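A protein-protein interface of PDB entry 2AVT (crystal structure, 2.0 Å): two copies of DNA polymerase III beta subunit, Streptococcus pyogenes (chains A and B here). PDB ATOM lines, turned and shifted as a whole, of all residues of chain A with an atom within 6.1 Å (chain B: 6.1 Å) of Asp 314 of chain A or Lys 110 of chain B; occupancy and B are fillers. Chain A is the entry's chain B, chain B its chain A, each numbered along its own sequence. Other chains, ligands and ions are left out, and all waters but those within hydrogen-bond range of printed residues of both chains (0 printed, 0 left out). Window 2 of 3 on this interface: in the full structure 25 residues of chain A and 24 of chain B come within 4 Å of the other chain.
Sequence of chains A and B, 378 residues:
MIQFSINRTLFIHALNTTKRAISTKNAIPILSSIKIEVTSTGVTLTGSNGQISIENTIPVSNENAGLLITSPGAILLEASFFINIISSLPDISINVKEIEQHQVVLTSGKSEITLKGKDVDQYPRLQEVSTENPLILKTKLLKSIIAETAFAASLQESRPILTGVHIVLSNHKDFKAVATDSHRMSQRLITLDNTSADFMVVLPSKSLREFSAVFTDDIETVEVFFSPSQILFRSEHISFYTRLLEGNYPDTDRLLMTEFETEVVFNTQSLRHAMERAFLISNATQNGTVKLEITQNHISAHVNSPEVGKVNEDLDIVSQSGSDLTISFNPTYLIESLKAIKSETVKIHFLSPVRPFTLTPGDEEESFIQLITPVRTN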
ATOM      1  N   ILE A 299       2.275 -25.193 -20.319  1.00  0.00           N
ATOM      2  CA  ILE A 299       0.845 -24.899 -20.279  1.00  0.00           C
ATOM      3  C   ILE A 299       0.653 -23.663 -19.395  1.00  0.00           C
ATOM      4  O   ILE A 299       1.065 -23.669 -18.242  1.00  0.00           O
ATOM      5  CB  ILE A 299       0.066 -26.050 -19.609  1.00  0.00           C
ATOM      6  CG1 ILE A 299       0.542 -27.402 -20.156  1.00  0.00           C
ATOM      7  CG2 ILE A 299      -1.435 -25.855 -19.809  1.00  0.00           C
ATOM      8  CD1 ILE A 299       0.246 -27.619 -21.620  1.00  0.00           C
ATOM      9  N   SER A 300       0.042 -22.609 -19.918  1.00  0.00           N
ATOM     10  CA  SER A 300      -0.172 -21.423 -19.098  1.00  0.00           C
ATOM     11  C   SER A 300      -1.559 -20.822 -19.275  1.00  0.00           C
ATOM     12  O   SER A 300      -2.197 -20.990 -20.326  1.00  0.00           O
ATOM     13  CB  SER A 300       0.902 -20.370 -19.395  1.00  0.00           C
ATOM     14  OG  SER A 300       0.947 -20.048 -20.773  1.00  0.00           O
ATOM     15  N   ALA A 301      -2.027 -20.144 -18.227  1.00  0.00           N
ATOM     16  CA  ALA A 301      -3.328 -19.476 -18.230  1.00  0.00           C
ATOM     17  C   ALA A 301      -3.070 -17.975 -18.164  1.00  0.00           C
ATOM     18  O   ALA A 301      -2.193 -17.504 -17.431  1.00  0.00           O
ATOM     19  CB  ALA A 301      -4.169 -19.926 -17.040  1.00  0.00           C
ATOM     20  N   ASN A 312      -1.060 -14.353 -15.120  1.00  0.00           N
ATOM     21  CA  ASN A 312      -0.169 -15.120 -15.971  1.00  0.00           C
ATOM     22  C   ASN A 312       0.272 -16.252 -15.070  1.00  0.00           C
ATOM     23  O   ASN A 312       1.024 -16.035 -14.122  1.00  0.00           O
ATOM     24  CB  ASN A 312       1.047 -14.305 -16.392  1.00  0.00           C
ATOM     25  CG  ASN A 312       2.004 -15.115 -17.239  1.00  0.00           C
ATOM     26  OD1 ASN A 312       2.355 -16.250 -16.887  1.00  0.00           O
ATOM     27  ND2 ASN A 312       2.433 -14.545 -18.360  1.00  0.00           N
ATOM     28  N   GLU A 313      -0.206 -17.459 -15.346  1.00  0.00           N
ATOM     29  CA  GLU A 313       0.144 -18.579 -14.502  1.00  0.00           C
ATOM     30  C   GLU A 313       0.550 -19.844 -15.244  1.00  0.00           C
ATOM     31  O   GLU A 313      -0.165 -20.291 -16.144  1.00  0.00           O
ATOM     32  CB  GLU A 313      -1.034 -18.909 -13.581  1.00  0.00           C
ATOM     33  CG  GLU A 313      -0.732 -20.021 -12.581  1.00  0.00           C
ATOM     34  CD  GLU A 313      -1.853 -20.234 -11.595  1.00  0.00           C
ATOM     35  OE1 GLU A 313      -2.517 -19.242 -11.238  1.00  0.00           O
ATOM     36  OE2 GLU A 313      -2.062 -21.384 -11.160  1.00  0.00           O
ATOM     37  N   ASP A 314       1.692 -20.415 -14.853  1.00  0.00           N
ATOM     38  CA  ASP A 314       2.175 -21.665 -15.448  1.00  0.00           C
ATOM     39  C   ASP A 314       1.500 -22.826 -14.722  1.00  0.00           C
ATOM     40  O   ASP A 314       1.431 -22.854 -13.485  1.00  0.00           O
ATOM     41  CB  ASP A 314       3.705 -21.789 -15.331  1.00  0.00           C
ATOM     42  CG  ASP A 314       4.449 -20.798 -16.217  1.00  0.00           C
ATOM     43  OD1 ASP A 314       4.026 -20.572 -17.371  1.00  0.00           O
ATOM     44  OD2 ASP A 314       5.478 -20.248 -15.766  1.00  0.00           O
ATOM     45  N   LEU A 315       1.003 -23.789 -15.490  1.00  0.00           N
ATOM     46  CA  LEU A 315       0.296 -24.929 -14.914  1.00  0.00           C
ATOM     47  C   LEU A 315       1.036 -26.261 -14.985  1.00  0.00           C
ATOM     48  O   LEU A 315       1.697 -26.565 -15.980  1.00  0.00           O
ATOM     49  CB  LEU A 315      -1.069 -25.100 -15.606  1.00  0.00           C
ATOM     50  CG  LEU A 315      -1.997 -23.882 -15.738  1.00  0.00           C
ATOM     51  CD1 LEU A 315      -3.315 -24.330 -16.350  1.00  0.00           C
ATOM     52  CD2 LEU A 315      -2.253 -23.253 -14.380  1.00  0.00           C
ATOM     53  N   ASP A 316       0.920 -27.049 -13.925  1.00  0.00           N
ATOM     54  CA  ASP A 316       1.517 -28.375 -13.895  1.00  0.00           C
ATOM     55  C   ASP A 316       0.466 -29.309 -14.488  1.00  0.00           C
ATOM     56  O   ASP A 316      -0.745 -29.088 -14.313  1.00  0.00           O
ATOM     57  CB  ASP A 316       1.815 -28.840 -12.462  1.00  0.00           C
ATOM     58  CG  ASP A 316       2.966 -28.085 -11.817  1.00  0.00           C
ATOM     59  OD1 ASP A 316       3.839 -27.561 -12.538  1.00  0.00           O
ATOM     60  OD2 ASP A 316       3.002 -28.039 -10.574  1.00  0.00           O
ATOM     61  N   PRO B  90      -1.560 -19.803  -4.485  1.00  0.00           N
ATOM     62  CA  PRO B  90      -1.090 -21.164  -4.219  1.00  0.00           C
ATOM     63  C   PRO B  90      -0.014 -21.452  -3.166  1.00  0.00           C
ATOM     64  O   PRO B  90      -0.204 -22.332  -2.333  1.00  0.00           O
ATOM     65  CB  PRO B  90      -0.691 -21.654  -5.612  1.00  0.00           C
ATOM     66  CG  PRO B  90      -0.076 -20.425  -6.216  1.00  0.00           C
ATOM     67  CD  PRO B  90      -1.021 -19.301  -5.765  1.00  0.00           C
ATOM     68  N   ASP B  91       1.103 -20.732  -3.196  1.00  0.00           N
ATOM     69  CA  ASP B  91       2.182 -20.997  -2.245  1.00  0.00           C
ATOM     70  C   ASP B  91       2.133 -20.314  -0.884  1.00  0.00           C
ATOM     71  O   ASP B  91       1.476 -19.287  -0.695  1.00  0.00           O
ATOM     72  CB  ASP B  91       3.534 -20.709  -2.897  1.00  0.00           C
ATOM     73  CG  ASP B  91       4.086 -21.915  -3.640  1.00  0.00           C
ATOM     74  OD1 ASP B  91       3.359 -22.501  -4.480  1.00  0.00           O
ATOM     75  OD2 ASP B  91       5.255 -22.279  -3.386  1.00  0.00           O
ATOM     76  N   THR B 107       3.453 -12.478  -6.721  1.00  0.00           N
ATOM     77  CA  THR B 107       3.979 -13.752  -7.196  1.00  0.00           C
ATOM     78  C   THR B 107       3.964 -14.784  -6.083  1.00  0.00           C
ATOM     79  O   THR B 107       4.490 -14.554  -4.984  1.00  0.00           O
ATOM     80  CB  THR B 107       5.420 -13.607  -7.715  1.00  0.00           C
ATOM     81  OG1 THR B 107       5.441 -12.666  -8.792  1.00  0.00           O
ATOM     82  CG2 THR B 107       5.948 -14.949  -8.224  1.00  0.00           C
ATOM     83  N   SER B 108       3.329 -15.914  -6.361  1.00  0.00           N
ATOM     84  CA  SER B 108       3.230 -17.002  -5.405  1.00  0.00           C
ATOM     85  C   SER B 108       3.291 -18.292  -6.202  1.00  0.00           C
ATOM     86  O   SER B 108       2.337 -18.652  -6.888  1.00  0.00           O
ATOM     87  CB  SER B 108       1.908 -16.931  -4.639  1.00  0.00           C
ATOM     88  OG  SER B 108       1.810 -17.982  -3.695  1.00  0.00           O
ATOM     89  N   GLY B 109       4.417 -18.988  -6.104  1.00  0.00           N
ATOM     90  CA  GLY B 109       4.570 -20.225  -6.844  1.00  0.00           C
ATOM     91  C   GLY B 109       4.660 -19.884  -8.315  1.00  0.00           C
ATOM     92  O   GLY B 109       5.361 -18.951  -8.699  1.00  0.00           O
ATOM     93  N   LYS B 110       3.921 -20.615  -9.137  1.00  0.00           N
ATOM     94  CA  LYS B 110       3.925 -20.398 -10.578  1.00  0.00           C
ATOM     95  C   LYS B 110       2.880 -19.378 -10.996  1.00  0.00           C
ATOM     96  O   LYS B 110       2.683 -19.147 -12.189  1.00  0.00           O
ATOM     97  CB  LYS B 110       3.639 -21.715 -11.294  1.00  0.00           C
ATOM     98  CG  LYS B 110       4.709 -22.763 -11.090  1.00  0.00           C
ATOM     99  CD  LYS B 110       4.097 -24.147 -11.117  1.00  0.00           C
ATOM    100  CE  LYS B 110       3.009 -24.247 -10.057  1.00  0.00           C
ATOM    101  NZ  LYS B 110       2.581 -25.650  -9.820  1.00  0.00           N
ATOM    102  N   SER B 111       2.215 -18.770 -10.016  1.00  0.00           N
ATOM    103  CA  SER B 111       1.166 -17.801 -10.299  1.00  0.00           C
ATOM    104  C   SER B 111       1.606 -16.350 -10.146  1.00  0.00           C
ATOM    105  O   SER B 111       2.161 -15.960  -9.114  1.00  0.00           O
ATOM    106  CB  SER B 111      -0.045 -18.071  -9.392  1.00  0.00           C
ATOM    107  OG  SER B 111      -1.154 -17.272  -9.766  1.00  0.00           O
ATOM    108  N   GLU B 112       1.381 -15.563 -11.192  1.00  0.00           N
ATOM    109  CA  GLU B 112       1.714 -14.145 -11.181  1.00  0.00           C
ATOM    110  C   GLU B 112       0.464 -13.320 -11.495  1.00  0.00           C
ATOM    111  O   GLU B 112      -0.089 -13.399 -12.600  1.00  0.00           O
ATOM    112  CB  GLU B 112       2.788 -13.816 -12.206  1.00  0.00           C
ATOM    113  CG  GLU B 112       3.066 -12.322 -12.259  1.00  0.00           C
ATOM    114  CD  GLU B 112       4.071 -11.940 -13.315  1.00  0.00           C
ATOM    115  OE1 GLU B 112       5.276 -12.173 -13.101  1.00  0.00           O
ATOM    116  OE2 GLU B 112       3.651 -11.410 -14.368  1.00  0.00           O
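OE1 of Glu 313 of chain A lies within hydrogen-bond range of OG of Ser 111 of chain B.
The backbone NH (N) of Asn 312 of chain A is in hydrogen-bond range of the backbone carbonyl oxygen (O) of Glu 112 of chain B (2.9 Å).
The backbone carbonyl oxygen (O) of Lys 110 of chain B is in hydrogen-bond range of the backbone NH (N) of Asp 314 of chain A (3.1 Å).
The side-chain amino group (NZ) of Lys 110 of chain B lies within salt-bridge range of the side-chain carboxylate (OD2) of Asp 316 of chain A, 2.5 Å away.
Of the 8 printed residues of chain B, 3 touch a printed residue of chain A.
Among the printed residues, 5 pairs touch across the chains.
O of Glu 313 of chain A is in hydrogen-bond range of N of Ala 301 of chain A (2.8 Å).
No position is printed for both chains.
Of the 5 pairs that touch across the chains among the printed residues, none has its exchanged pair printed and touching as well.
Ser 300 of chain A touches none of the printed residues of chain B.
Ala 301 of chain A touches none of the printed residues of chain B.
Of the printed residues of chain B, Asn 312 of chain A touches Glu 112 (2.9 Å).
Of the printed residues of chain B, Glu 313 of chain A touches Lys 110 and Ser 111.
Of the printed residues of chain B, Asp 314 of chain A touches Lys 110 (3.1 Å).
Of the printed residues of chain A, Ser 111 of chain B touches Glu 313.
The nearest residue of chain B that does not touch Asp 314 of chain A is Ser 111 of chain B (5.1 Å).
The nearest residue of chain A that does not touch Lys 110 of chain B is Asn 312 of chain A (4.02 Å).
The nearest printed residue of chain B that does not touch Glu 313 of chain A is Glu 112 of chain B (4.6 Å).
Among the printed residues, pairs that only touch across the chains: Glu 313 of chain A with Lys 110 of chain B (3.5 Å).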
